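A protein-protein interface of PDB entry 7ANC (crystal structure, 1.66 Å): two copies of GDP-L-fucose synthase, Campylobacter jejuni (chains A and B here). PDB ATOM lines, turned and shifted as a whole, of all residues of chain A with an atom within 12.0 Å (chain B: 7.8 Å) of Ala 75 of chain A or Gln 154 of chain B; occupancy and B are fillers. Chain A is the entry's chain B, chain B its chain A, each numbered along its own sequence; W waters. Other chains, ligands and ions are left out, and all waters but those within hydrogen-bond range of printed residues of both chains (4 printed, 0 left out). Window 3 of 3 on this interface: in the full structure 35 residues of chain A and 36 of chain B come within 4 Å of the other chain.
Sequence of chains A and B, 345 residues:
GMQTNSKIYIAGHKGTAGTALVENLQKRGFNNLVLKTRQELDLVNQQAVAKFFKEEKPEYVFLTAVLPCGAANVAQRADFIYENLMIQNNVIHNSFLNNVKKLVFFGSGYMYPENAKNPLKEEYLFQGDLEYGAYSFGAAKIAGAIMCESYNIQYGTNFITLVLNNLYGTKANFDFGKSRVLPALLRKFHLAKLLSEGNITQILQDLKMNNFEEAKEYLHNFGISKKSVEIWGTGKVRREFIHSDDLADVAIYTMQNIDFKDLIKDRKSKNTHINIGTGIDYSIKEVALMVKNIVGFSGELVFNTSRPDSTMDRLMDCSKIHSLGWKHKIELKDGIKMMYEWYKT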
ATOM      1  N   LEU A  67      -0.484 -36.504 -12.760  1.00  0.00           N
ATOM      2  CA  LEU A  67       0.341 -35.849 -13.782  1.00  0.00           C
ATOM      3  C   LEU A  67       1.700 -36.539 -13.751  1.00  0.00           C
ATOM      4  O   LEU A  67       2.500 -36.281 -12.856  1.00  0.00           O
ATOM      5  CB  LEU A  67       0.442 -34.330 -13.530  1.00  0.00           C
ATOM      6  CG  LEU A  67       1.458 -33.624 -14.477  1.00  0.00           C
ATOM      7  CD1 LEU A  67       1.060 -33.732 -15.962  1.00  0.00           C
ATOM      8  CD2 LEU A  67       1.628 -32.170 -14.058  1.00  0.00           C
ATOM      9  N   PRO A  68       2.024 -37.434 -14.720  1.00  0.00           N
ATOM     10  CA  PRO A  68       3.273 -38.197 -14.669  1.00  0.00           C
ATOM     11  C   PRO A  68       4.456 -37.392 -15.210  1.00  0.00           C
ATOM     12  O   PRO A  68       4.290 -36.517 -16.065  1.00  0.00           O
ATOM     13  CB  PRO A  68       2.985 -39.369 -15.605  1.00  0.00           C
ATOM     14  CG  PRO A  68       2.076 -38.785 -16.636  1.00  0.00           C
ATOM     15  CD  PRO A  68       1.223 -37.746 -15.917  1.00  0.00           C
ATOM     16  N   CYS A  69       5.628 -37.693 -14.651  1.00  0.00           N
ATOM     17  CA  CYS A  69       6.928 -37.107 -14.946  1.00  0.00           C
ATOM     18  C   CYS A  69       7.616 -38.071 -15.904  1.00  0.00           C
ATOM     19  O   CYS A  69       7.726 -39.242 -15.582  1.00  0.00           O
ATOM     20  CB  CYS A  69       7.757 -37.014 -13.631  1.00  0.00           C
ATOM     21  SG  CYS A  69       9.384 -36.300 -13.884  1.00  0.00           S
ATOM     22  N   GLY A  70       8.055 -37.583 -17.072  1.00  0.00           N
ATOM     23  CA  GLY A  70       8.883 -38.351 -18.008  1.00  0.00           C
ATOM     24  C   GLY A  70       9.978 -37.468 -18.615  1.00  0.00           C
ATOM     25  O   GLY A  70      10.094 -36.284 -18.272  1.00  0.00           O
ATOM     26  N   ALA A  71      10.745 -38.031 -19.557  1.00  0.00           N
ATOM     27  CA  ALA A  71      11.792 -37.303 -20.283  1.00  0.00           C
ATOM     28  C   ALA A  71      11.277 -36.096 -21.097  1.00  0.00           C
ATOM     29  O   ALA A  71      11.903 -35.039 -21.110  1.00  0.00           O
ATOM     30  CB  ALA A  71      12.567 -38.251 -21.192  1.00  0.00           C
ATOM     31  N   ALA A  72      10.133 -36.266 -21.765  1.00  0.00           N
ATOM     32  CA  ALA A  72       9.548 -35.222 -22.606  1.00  0.00           C
ATOM     33  C   ALA A  72       8.991 -33.988 -21.850  1.00  0.00           C
ATOM     34  O   ALA A  72       8.945 -32.905 -22.427  1.00  0.00           O
ATOM     35  CB  ALA A  72       8.457 -35.813 -23.490  1.00  0.00           C
ATOM     36  N   ASN A  73       8.530 -34.155 -20.595  1.00  0.00           N
ATOM     37  CA  ASN A  73       7.928 -33.014 -19.850  1.00  0.00           C
ATOM     38  C   ASN A  73       8.638 -32.627 -18.539  1.00  0.00           C
ATOM     39  O   ASN A  73       8.046 -31.956 -17.713  1.00  0.00           O
ATOM     40  CB  ASN A  73       6.439 -33.261 -19.587  1.00  0.00           C
ATOM     41  CG  ASN A  73       6.177 -34.417 -18.603  1.00  0.00           C
ATOM     42  OD1 ASN A  73       7.099 -35.159 -18.215  1.00  0.00           O
ATOM     43  ND2 ASN A  73       4.911 -34.593 -18.227  1.00  0.00           N
ATOM     44  N   VAL A  74       9.906 -33.024 -18.390  1.00  0.00           N
ATOM     45  CA  VAL A  74      10.677 -32.834 -17.166  1.00  0.00           C
ATOM     46  C   VAL A  74      10.796 -31.354 -16.747  1.00  0.00           C
ATOM     47  O   VAL A  74      11.049 -31.047 -15.558  1.00  0.00           O
ATOM     48  CB  VAL A  74      12.066 -33.527 -17.239  1.00  0.00           C
ATOM     49  CG1 VAL A  74      13.067 -32.715 -18.072  1.00  0.00           C
ATOM     50  CG2 VAL A  74      12.619 -33.767 -15.835  1.00  0.00           C
ATOM     51  N   ALA A  75      10.554 -30.427 -17.689  1.00  0.00           N
ATOM     52  CA  ALA A  75      10.541 -28.993 -17.365  1.00  0.00           C
ATOM     53  C   ALA A  75       9.416 -28.548 -16.418  1.00  0.00           C
ATOM     54  O   ALA A  75       9.488 -27.450 -15.822  1.00  0.00           O
ATOM     55  CB  ALA A  75      10.482 -28.162 -18.641  1.00  0.00           C
ATOM     56  N   GLN A  76       8.389 -29.387 -16.267  1.00  0.00           N
ATOM     57  CA  GLN A  76       7.161 -29.033 -15.518  1.00  0.00           C
ATOM     58  C   GLN A  76       7.312 -29.251 -13.992  1.00  0.00           C
ATOM     59  O   GLN A  76       6.406 -29.778 -13.341  1.00  0.00           O
ATOM     60  CB  GLN A  76       5.938 -29.772 -16.080  1.00  0.00           C
ATOM     61  CG  GLN A  76       5.534 -29.274 -17.491  1.00  0.00           C
ATOM     62  CD  GLN A  76       4.242 -29.885 -17.980  1.00  0.00           C
ATOM     63  OE1 GLN A  76       4.281 -30.694 -18.885  1.00  0.00           O
ATOM     64  NE2 GLN A  76       3.075 -29.530 -17.352  1.00  0.00           N
ATOM     65  N   ARG A  77       8.448 -28.786 -13.444  1.00  0.00           N
ATOM     66  CA  ARG A  77       8.867 -29.055 -12.055  1.00  0.00           C
ATOM     67  C   ARG A  77       7.831 -28.594 -11.009  1.00  0.00           C
ATOM     68  O   ARG A  77       7.545 -29.310 -10.034  1.00  0.00           O
ATOM     69  CB  ARG A  77      10.222 -28.387 -11.760  1.00  0.00           C
ATOM     70  CG  ARG A  77      10.995 -29.037 -10.624  1.00  0.00           C
ATOM     71  CD  ARG A  77      12.374 -28.442 -10.539  1.00  0.00           C
ATOM     72  NE  ARG A  77      13.295 -29.066  -9.595  1.00  0.00           N
ATOM     73  CZ  ARG A  77      13.937 -30.201  -9.788  1.00  0.00           C
ATOM     74  NH1 ARG A  77      13.736 -30.911 -10.881  1.00  0.00           N
ATOM     75  NH2 ARG A  77      14.790 -30.639  -8.890  1.00  0.00           N
ATOM     76  N   ALA A  78       7.252 -27.405 -11.209  1.00  0.00           N
ATOM     77  CA  ALA A  78       6.199 -26.897 -10.299  1.00  0.00           C
ATOM     78  C   ALA A  78       4.885 -27.643 -10.440  1.00  0.00           C
ATOM     79  O   ALA A  78       4.263 -28.003  -9.439  1.00  0.00           O
ATOM     80  CB  ALA A  78       5.958 -25.383 -10.484  1.00  0.00           C
ATOM     81  N   ASP A  79       4.478 -27.908 -11.688  1.00  0.00           N
ATOM     82  CA  ASP A  79       3.211 -28.589 -11.958  1.00  0.00           C
ATOM     83  C   ASP A  79       3.195 -30.016 -11.335  1.00  0.00           C
ATOM     84  O   ASP A  79       2.171 -30.454 -10.770  1.00  0.00           O
ATOM     85  CB  ASP A  79       2.948 -28.686 -13.454  1.00  0.00           C
ATOM     86  CG  ASP A  79       2.904 -27.344 -14.181  1.00  0.00           C
ATOM     87  OD1 ASP A  79       2.721 -26.276 -13.589  1.00  0.00           O
ATOM     88  OD2 ASP A  79       3.101 -27.383 -15.407  1.00  0.00           O
ATOM     89  N   PHE A  80       4.332 -30.724 -11.398  1.00  0.00           N
ATOM     90  CA  PHE A  80       4.422 -32.083 -10.819  1.00  0.00           C
ATOM     91  C   PHE A  80       4.083 -32.095  -9.330  1.00  0.00           C
ATOM     92  O   PHE A  80       3.435 -33.054  -8.857  1.00  0.00           O
ATOM     93  CB  PHE A  80       5.792 -32.744 -10.978  1.00  0.00           C
ATOM     94  CG  PHE A  80       6.203 -33.003 -12.408  1.00  0.00           C
ATOM     95  CD1 PHE A  80       5.297 -33.546 -13.321  1.00  0.00           C
ATOM     96  CD2 PHE A  80       7.492 -32.725 -12.830  1.00  0.00           C
ATOM     97  CE1 PHE A  80       5.663 -33.762 -14.656  1.00  0.00           C
ATOM     98  CE2 PHE A  80       7.858 -32.940 -14.147  1.00  0.00           C
ATOM     99  CZ  PHE A  80       6.941 -33.449 -15.058  1.00  0.00           C
ATOM    100  N   ILE A  81       4.588 -31.101  -8.578  1.00  0.00           N
ATOM    101  CA  ILE A  81       4.291 -31.043  -7.141  1.00  0.00           C
ATOM    102  C   ILE A  81       2.885 -30.474  -6.846  1.00  0.00           C
ATOM    103  O   ILE A  81       2.097 -31.077  -6.102  1.00  0.00           O
ATOM    104  CB  ILE A  81       5.462 -30.504  -6.272  1.00  0.00           C
ATOM    105  CG1 ILE A  81       5.113 -30.593  -4.760  1.00  0.00           C
ATOM    106  CG2 ILE A  81       5.901 -29.078  -6.684  1.00  0.00           C
ATOM    107  CD1 ILE A  81       6.298 -30.370  -3.862  1.00  0.00           C
ATOM    108  N   TYR A  82       2.534 -29.327  -7.440  1.00  0.00           N
ATOM    109  CA  TYR A  82       1.227 -28.711  -7.147  1.00  0.00           C
ATOM    110  C   TYR A  82       0.032 -29.618  -7.566  1.00  0.00           C
ATOM    111  O   TYR A  82      -0.869 -29.873  -6.756  1.00  0.00           O
ATOM    112  CB  TYR A  82       1.103 -27.330  -7.807  1.00  0.00           C
ATOM    113  CG  TYR A  82      -0.281 -26.745  -7.686  1.00  0.00           C
ATOM    114  CD1 TYR A  82      -0.751 -26.286  -6.459  1.00  0.00           C
ATOM    115  CD2 TYR A  82      -1.182 -26.750  -8.774  1.00  0.00           C
ATOM    116  CE1 TYR A  82      -2.036 -25.763  -6.330  1.00  0.00           C
ATOM    117  CE2 TYR A  82      -2.485 -26.242  -8.637  1.00  0.00           C
ATOM    118  CZ  TYR A  82      -2.899 -25.763  -7.391  1.00  0.00           C
ATOM    119  OH  TYR A  82      -4.180 -25.247  -7.183  1.00  0.00           O
ATOM    120  N   GLU A  83       0.026 -30.071  -8.829  1.00  0.00           N
ATOM    121  CA  GLU A  83      -1.128 -30.849  -9.340  1.00  0.00           C
ATOM    122  C   GLU A  83      -1.312 -32.175  -8.588  1.00  0.00           C
ATOM    123  O   GLU A  83      -2.444 -32.529  -8.168  1.00  0.00           O
ATOM    124  CB  GLU A  83      -1.063 -31.046 -10.849  1.00  0.00           C
ATOM    125  CG  GLU A  83      -1.141 -29.691 -11.570  1.00  0.00           C
ATOM    126  CD  GLU A  83      -1.307 -29.767 -13.085  1.00  0.00           C
ATOM    127  OE1 GLU A  83      -1.837 -30.775 -13.599  1.00  0.00           O
ATOM    128  OE2 GLU A  83      -0.884 -28.803 -13.746  1.00  0.00           O
ATOM    129  N   ASN A  84      -0.211 -32.893  -8.355  1.00  0.00           N
ATOM    130  CA  ASN A  84      -0.275 -34.164  -7.643  1.00  0.00           C
ATOM    131  C   ASN A  84      -0.627 -34.035  -6.163  1.00  0.00           C
ATOM    132  O   ASN A  84      -1.485 -34.782  -5.638  1.00  0.00           O
ATOM    133  CB  ASN A  84       0.975 -35.017  -7.884  1.00  0.00           C
ATOM    134  CG  ASN A  84       1.036 -35.520  -9.325  1.00  0.00           C
ATOM    135  OD1 ASN A  84       0.033 -36.094  -9.846  1.00  0.00           O
ATOM    136  ND2 ASN A  84       2.148 -35.247 -10.011  1.00  0.00           N
ATOM    137  N   GLU A 131      16.422 -38.426  -6.902  1.00  0.00           N
ATOM    138  CA  GLU A 131      16.974 -38.131  -8.275  1.00  0.00           C
ATOM    139  C   GLU A 131      16.530 -36.718  -8.727  1.00  0.00           C
ATOM    140  O   GLU A 131      15.393 -36.321  -8.501  1.00  0.00           O
ATOM    141  CB  GLU A 131      16.536 -39.184  -9.278  1.00  0.00           C
ATOM    142  CG  GLU A 131      17.283 -39.144 -10.632  1.00  0.00           C
ATOM    143  CD  GLU A 131      16.642 -38.185 -11.649  1.00  0.00           C
ATOM    144  OE1 GLU A 131      15.376 -38.121 -11.677  1.00  0.00           O
ATOM    145  OE2 GLU A 131      17.383 -37.471 -12.415  1.00  0.00           O
ATOM    146  N   TYR A 132      17.440 -35.947  -9.345  1.00  0.00           N
ATOM    147  CA  TYR A 132      17.182 -34.534  -9.627  1.00  0.00           C
ATOM    148  C   TYR A 132      15.945 -34.261 -10.510  1.00  0.00           C
ATOM    149  O   TYR A 132      15.127 -33.379 -10.209  1.00  0.00           O
ATOM    150  CB  TYR A 132      18.454 -33.844 -10.227  1.00  0.00           C
ATOM    151  CG  TYR A 132      18.277 -32.352 -10.301  1.00  0.00           C
ATOM    152  CD1 TYR A 132      18.580 -31.552  -9.201  1.00  0.00           C
ATOM    153  CD2 TYR A 132      17.769 -31.741 -11.432  1.00  0.00           C
ATOM    154  CE1 TYR A 132      18.381 -30.183  -9.210  1.00  0.00           C
ATOM    155  CE2 TYR A 132      17.556 -30.346 -11.461  1.00  0.00           C
ATOM    156  CZ  TYR A 132      17.879 -29.575 -10.359  1.00  0.00           C
ATOM    157  OH  TYR A 132      17.671 -28.207 -10.357  1.00  0.00           O
ATOM    158  N   GLY A 133      15.821 -34.961 -11.637  1.00  0.00           N
ATOM    159  CA  GLY A 133      14.728 -34.724 -12.570  1.00  0.00           C
ATOM    160  C   GLY A 133      13.346 -34.962 -11.951  1.00  0.00           C
ATOM    161  O   GLY A 133      12.387 -34.230 -12.203  1.00  0.00           O
ATOM    162  N   ALA A 134      13.266 -36.031 -11.160  1.00  0.00           N
ATOM    163  CA  ALA A 134      12.037 -36.479 -10.499  1.00  0.00           C
ATOM    164  C   ALA A 134      11.875 -35.957  -9.047  1.00  0.00           C
ATOM    165  O   ALA A 134      10.955 -36.419  -8.301  1.00  0.00           O
ATOM    166  CB  ALA A 134      11.964 -37.993 -10.525  1.00  0.00           C
ATOM    167  N   TYR A 135      12.722 -35.003  -8.637  1.00  0.00           N
ATOM    168  CA  TYR A 135      12.749 -34.527  -7.249  1.00  0.00           C
ATOM    169  C   TYR A 135      11.375 -34.016  -6.733  1.00  0.00           C
ATOM    170  O   TYR A 135      10.948 -34.357  -5.624  1.00  0.00           O
ATOM    171  CB  TYR A 135      13.780 -33.377  -7.179  1.00  0.00           C
ATOM    172  CG  TYR A 135      14.069 -32.729  -5.828  1.00  0.00           C
ATOM    173  CD1 TYR A 135      14.903 -33.343  -4.902  1.00  0.00           C
ATOM    174  CD2 TYR A 135      13.582 -31.451  -5.517  1.00  0.00           C
ATOM    175  CE1 TYR A 135      15.218 -32.707  -3.691  1.00  0.00           C
ATOM    176  CE2 TYR A 135      13.901 -30.813  -4.311  1.00  0.00           C
ATOM    177  CZ  TYR A 135      14.705 -31.458  -3.395  1.00  0.00           C
ATOM    178  OH  TYR A 135      15.041 -30.834  -2.202  1.00  0.00           O
ATOM    179  N   SER A 136      10.713 -33.146  -7.514  1.00  0.00           N
ATOM    180  CA  SER A 136       9.424 -32.580  -7.088  1.00  0.00           C
ATOM    181  C   SER A 136       8.245 -33.586  -7.149  1.00  0.00           C
ATOM    182  O   SER A 136       7.392 -33.619  -6.249  1.00  0.00           O
ATOM    183  CB  SER A 136       9.130 -31.290  -7.820  1.00  0.00           C
ATOM    184  OG  SER A 136       8.853 -31.511  -9.176  1.00  0.00           O
ATOM    185  N   PHE A 137       8.253 -34.465  -8.150  1.00  0.00           N
ATOM    186  CA  PHE A 137       7.290 -35.550  -8.312  1.00  0.00           C
ATOM    187  C   PHE A 137       7.436 -36.576  -7.150  1.00  0.00           C
ATOM    188  O   PHE A 137       6.456 -36.967  -6.495  1.00  0.00           O
ATOM    189  CB  PHE A 137       7.499 -36.230  -9.673  1.00  0.00           C
ATOM    190  CG  PHE A 137       6.623 -37.438  -9.899  1.00  0.00           C
ATOM    191  CD1 PHE A 137       5.331 -37.302 -10.379  1.00  0.00           C
ATOM    192  CD2 PHE A 137       7.099 -38.702  -9.650  1.00  0.00           C
ATOM    193  CE1 PHE A 137       4.522 -38.424 -10.589  1.00  0.00           C
ATOM    194  CE2 PHE A 137       6.296 -39.836  -9.826  1.00  0.00           C
ATOM    195  CZ  PHE A 137       5.016 -39.681 -10.302  1.00  0.00           C
ATOM    196  N   PHE B  96       1.200 -17.029  -7.736  1.00  0.00           N
ATOM    197  CA  PHE B  96       1.674 -17.206  -9.121  1.00  0.00           C
ATOM    198  C   PHE B  96       0.644 -16.772 -10.178  1.00  0.00           C
ATOM    199  O   PHE B  96       0.985 -16.008 -11.111  1.00  0.00           O
ATOM    200  CB  PHE B  96       2.173 -18.656  -9.345  1.00  0.00           C
ATOM    201  CG  PHE B  96       2.258 -19.083 -10.793  1.00  0.00           C
ATOM    202  CD1 PHE B  96       3.242 -18.598 -11.622  1.00  0.00           C
ATOM    203  CD2 PHE B  96       1.335 -19.994 -11.305  1.00  0.00           C
ATOM    204  CE1 PHE B  96       3.301 -18.986 -12.966  1.00  0.00           C
ATOM    205  CE2 PHE B  96       1.395 -20.405 -12.644  1.00  0.00           C
ATOM    206  CZ  PHE B  96       2.390 -19.913 -13.462  1.00  0.00           C
ATOM    207  N   CYS B 148       8.076 -23.816  -3.334  1.00  0.00           N
ATOM    208  CA  CYS B 148       8.666 -22.492  -3.594  1.00  0.00           C
ATOM    209  C   CYS B 148       9.762 -22.604  -4.663  1.00  0.00           C
ATOM    210  O   CYS B 148       9.708 -21.906  -5.692  1.00  0.00           O
ATOM    211  CB  CYS B 148       9.224 -21.846  -2.337  1.00  0.00           C
ATOM    212  SG  CYS B 148       7.953 -21.211  -1.167  1.00  0.00           S
ATOM    213  N   GLU B 149      10.741 -23.492  -4.433  1.00  0.00           N
ATOM    214  CA  GLU B 149      11.867 -23.667  -5.338  1.00  0.00           C
ATOM    215  C   GLU B 149      11.441 -24.109  -6.735  1.00  0.00           C
ATOM    216  O   GLU B 149      11.982 -23.608  -7.749  1.00  0.00           O
ATOM    217  CB  GLU B 149      12.864 -24.688  -4.771  1.00  0.00           C
ATOM    218  CG  GLU B 149      14.130 -24.869  -5.613  1.00  0.00           C
ATOM    219  CD  GLU B 149      15.026 -25.928  -5.028  1.00  0.00           C
ATOM    220  OE1 GLU B 149      14.660 -27.147  -5.093  1.00  0.00           O
ATOM    221  OE2 GLU B 149      16.048 -25.515  -4.437  1.00  0.00           O
ATOM    222  N   SER B 150      10.440 -25.004  -6.807  1.00  0.00           N
ATOM    223  CA  SER B 150       9.977 -25.530  -8.070  1.00  0.00           C
ATOM    224  C   SER B 150       9.287 -24.452  -8.967  1.00  0.00           C
ATOM    225  O   SER B 150       9.510 -24.473 -10.187  1.00  0.00           O
ATOM    226  CB  SER B 150       9.058 -26.739  -7.872  1.00  0.00           C
ATOM    227  OG  SER B 150       9.765 -27.791  -7.190  1.00  0.00           O
ATOM    228  N   TYR B 151       8.458 -23.586  -8.366  1.00  0.00           N
ATOM    229  CA  TYR B 151       7.877 -22.429  -9.068  1.00  0.00           C
ATOM    230  C   TYR B 151       9.018 -21.504  -9.559  1.00  0.00           C
ATOM    231  O   TYR B 151       9.006 -21.028 -10.716  1.00  0.00           O
ATOM    232  CB  TYR B 151       6.817 -21.695  -8.179  1.00  0.00           C
ATOM    233  CG  TYR B 151       5.447 -22.343  -8.293  1.00  0.00           C
ATOM    234  CD1 TYR B 151       5.115 -23.481  -7.555  1.00  0.00           C
ATOM    235  CD2 TYR B 151       4.514 -21.882  -9.180  1.00  0.00           C
ATOM    236  CE1 TYR B 151       3.876 -24.113  -7.706  1.00  0.00           C
ATOM    237  CE2 TYR B 151       3.281 -22.492  -9.331  1.00  0.00           C
ATOM    238  CZ  TYR B 151       2.969 -23.624  -8.590  1.00  0.00           C
ATOM    239  OH  TYR B 151       1.749 -24.278  -8.778  1.00  0.00           O
ATOM    240  N   ASN B 152      10.028 -21.292  -8.717  1.00  0.00           N
ATOM    241  CA  ASN B 152      11.135 -20.390  -9.067  1.00  0.00           C
ATOM    242  C   ASN B 152      11.879 -20.936 -10.332  1.00  0.00           C
ATOM    243  O   ASN B 152      12.243 -20.172 -11.232  1.00  0.00           O
ATOM    244  CB  ASN B 152      12.113 -20.181  -7.912  1.00  0.00           C
ATOM    245  CG  ASN B 152      11.496 -19.498  -6.689  1.00  0.00           C
ATOM    246  OD1 ASN B 152      10.400 -18.888  -6.758  1.00  0.00           O
ATOM    247  ND2 ASN B 152      12.214 -19.595  -5.532  1.00  0.00           N
ATOM    248  N   ILE B 153      12.060 -22.268 -10.394  1.00  0.00           N
ATOM    249  CA  ILE B 153      12.764 -22.918 -11.497  1.00  0.00           C
ATOM    250  C   ILE B 153      11.937 -22.938 -12.778  1.00  0.00           C
ATOM    251  O   ILE B 153      12.430 -22.475 -13.825  1.00  0.00           O
ATOM    252  CB  ILE B 153      13.276 -24.349 -11.124  1.00  0.00           C
ATOM    253  CG1 ILE B 153      14.364 -24.227 -10.056  1.00  0.00           C
ATOM    254  CG2 ILE B 153      13.799 -25.105 -12.360  1.00  0.00           C
ATOM    255  CD1 ILE B 153      14.802 -25.554  -9.401  1.00  0.00           C
ATOM    256  N   GLN B 154      10.699 -23.455 -12.714  1.00  0.00           N
ATOM    257  CA  GLN B 154       9.870 -23.626 -13.910  1.00  0.00           C
ATOM    258  C   GLN B 154       9.387 -22.284 -14.463  1.00  0.00           C
ATOM    259  O   GLN B 154       9.393 -22.080 -15.670  1.00  0.00           O
ATOM    260  CB  GLN B 154       8.644 -24.549 -13.675  1.00  0.00           C
ATOM    261  CG  GLN B 154       7.707 -24.635 -14.865  1.00  0.00           C
ATOM    262  CD  GLN B 154       6.576 -25.644 -14.722  1.00  0.00           C
ATOM    263  OE1 GLN B 154       6.409 -26.318 -13.673  1.00  0.00           O
ATOM    264  NE2 GLN B 154       5.749 -25.750 -15.789  1.00  0.00           N
ATOM    265  N   TYR B 155       8.964 -21.383 -13.573  1.00  0.00           N
ATOM    266  CA  TYR B 155       8.242 -20.176 -13.958  1.00  0.00           C
ATOM    267  C   TYR B 155       8.958 -18.847 -13.659  1.00  0.00           C
ATOM    268  O   TYR B 155       8.444 -17.766 -13.941  1.00  0.00           O
ATOM    269  CB  TYR B 155       6.855 -20.170 -13.316  1.00  0.00           C
ATOM    270  CG  TYR B 155       5.875 -21.236 -13.758  1.00  0.00           C
ATOM    271  CD1 TYR B 155       5.403 -21.279 -15.051  1.00  0.00           C
ATOM    272  CD2 TYR B 155       5.368 -22.185 -12.854  1.00  0.00           C
ATOM    273  CE1 TYR B 155       4.471 -22.222 -15.460  1.00  0.00           C
ATOM    274  CE2 TYR B 155       4.407 -23.142 -13.247  1.00  0.00           C
ATOM    275  CZ  TYR B 155       3.966 -23.159 -14.569  1.00  0.00           C
ATOM    276  OH  TYR B 155       3.001 -24.066 -15.019  1.00  0.00           O
ATOM    277  N   GLY B 156      10.140 -18.905 -13.046  1.00  0.00           N
ATOM    278  CA  GLY B 156      10.864 -17.702 -12.679  1.00  0.00           C
ATOM    279  C   GLY B 156      10.184 -16.811 -11.657  1.00  0.00           C
ATOM    280  O   GLY B 156      10.366 -15.567 -11.655  1.00  0.00           O
ATOM    281  N   THR B 157       9.411 -17.428 -10.744  1.00  0.00           N
ATOM    282  CA  THR B 157       8.871 -16.699  -9.601  1.00  0.00           C
ATOM    283  C   THR B 157      10.011 -16.349  -8.622  1.00  0.00           C
ATOM    284  O   THR B 157      11.156 -16.781  -8.808  1.00  0.00           O
ATOM    285  CB  THR B 157       7.764 -17.511  -8.884  1.00  0.00           C
ATOM    286  OG1 THR B 157       8.283 -18.813  -8.584  1.00  0.00           O
ATOM    287  CG2 THR B 157       6.575 -17.682  -9.765  1.00  0.00           C
ATOM    288  N   PHE B 260      15.938 -15.036  -5.671  1.00  0.00           N
ATOM    289  CA  PHE B 260      16.237 -16.393  -6.067  1.00  0.00           C
ATOM    290  C   PHE B 260      17.549 -16.478  -6.888  1.00  0.00           C
ATOM    291  O   PHE B 260      18.371 -17.380  -6.650  1.00  0.00           O
ATOM    292  CB  PHE B 260      15.069 -17.023  -6.855  1.00  0.00           C
ATOM    293  CG  PHE B 260      15.331 -18.426  -7.351  1.00  0.00           C
ATOM    294  CD1 PHE B 260      15.482 -19.491  -6.456  1.00  0.00           C
ATOM    295  CD2 PHE B 260      15.431 -18.694  -8.733  1.00  0.00           C
ATOM    296  CE1 PHE B 260      15.697 -20.796  -6.920  1.00  0.00           C
ATOM    297  CE2 PHE B 260      15.668 -19.989  -9.190  1.00  0.00           C
ATOM    298  CZ  PHE B 260      15.810 -21.028  -8.286  1.00  0.00           C
HETATM  299  O   HOH W   1      15.915 -28.764  -6.966  1.00  0.00           O
HETATM  300  O   HOH W   2      12.791 -27.940  -6.977  1.00  0.00           O
HETATM  301  O   HOH W   3       1.271 -25.706 -11.230  1.00  0.00           O
HETATM  302  O   HOH W   4      15.553 -28.113  -2.673  1.00  0.00           O
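NE2 of Gln 154 of chain B lies within hydrogen-bond range of OD2 of Asp 79 of chain A, 3.1 Å away. N of Ala 78 of chain A is in hydrogen-bond range of OE1 of Gln 154 of chain B (2.8 Å). O of Gln 76 of chain A lies close to OE1 of Gln 154 of chain B (3.5 Å). OE1 of Gln 154 of chain B is in hydrogen-bond range of N of Arg 77 of chain A, at 3.2 Å. The side-chain hydroxyl (OH) of Tyr 155 of chain B is in hydrogen-bond range of the side-chain carboxylate (OD1) of Asp 79 of chain A (2.6 Å).
NE2 of Gln 76 of chain A sits at hydrogen-bond distance from OD2 of Asp 79 of chain A (2.9 Å). The backbone carbonyl oxygen (O) of Tyr 151 of chain B sits at hydrogen-bond distance from the backbone NH (N) of Gly 156 of chain B (3.3 Å). The backbone carbonyl oxygen (O) of Arg 77 of chain A sits at hydrogen-bond distance from the side-chain hydroxyl (OG) of Ser 136 of chain A (2.7 Å).
Arg 77 of chain A touches Ser 150 of chain B. Ile 153 of chain B touches Arg 77 of chain A. Ala 78 of chain A touches Ser 150 of chain B (CB to O, 3.7 Å). Ala 78 of chain A touches Tyr 151 of chain B (CB to CD1, 3.6 Å). Tyr 82 of chain A touches Tyr 151 of chain B. Tyr 135 of chain A touches Glu 149 of chain B (CE2 to OE1, 3.8 Å).
Of the printed residues of chain A, Gln 154 of chain B touches Ala 75 (3.5 Å), Gln 76 (3.1 Å), Arg 77 (3.2 Å), Ala 78 (2.8 Å) and Asp 79 (3.1 Å). Ser 150 of chain B touches just these residues of chain A: Arg 77 (3.7 Å), Ala 78 (3.7 Å) and Ser 136 (3.6 Å). Tyr 151 of chain B touches just these residues of chain A: Ala 78 and Tyr 82. Ile 153 of chain B touches one residue of chain A. Of chain A, only Ala 78 and Asp 79 come within 4 Å of Tyr 155 of chain B. Of the printed residues of chain B, Arg 77 of chain A touches Ser 150 (3.7 Å), Ile 153 (3.8 Å) and Gln 154 (3.2 Å). The nearest residue of chain A that does not touch Gln 154 of chain B is Phe 80 of chain A (5.4 Å). The nearest printed residue of chain B that does not touch Gln 76 of chain A is Tyr 155 of chain B (5.9 Å).
Of the 25 printed residues of chain A, 8 touch a printed residue of chain B. Hydrophobic or aromatic side chains of chain A within 4 Å of the printed part of chain B: Ala 78, Tyr 82 and Tyr 135. Along chain B the printed residues that touch a printed residue of chain A span positions 149 to 155. Among the printed residues, 14 pairs touch across the chains.
No position is printed for both chains. Of the 14 pairs that touch across the chains among the printed residues, none has its exchanged pair printed and touching as well.
Water W4 lies within hydrogen-bond range of OE1 of Glu 149 of chain B (2.8 Å) and OH of Tyr 135 of chain A (2.8 Å). Water W1 lies within hydrogen-bond range of the side-chain carboxylate (OE1) of Glu 149 of chain B (2.8 Å) and the guanidinium group (NH2) of Arg 77 of chain A (2.9 Å).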
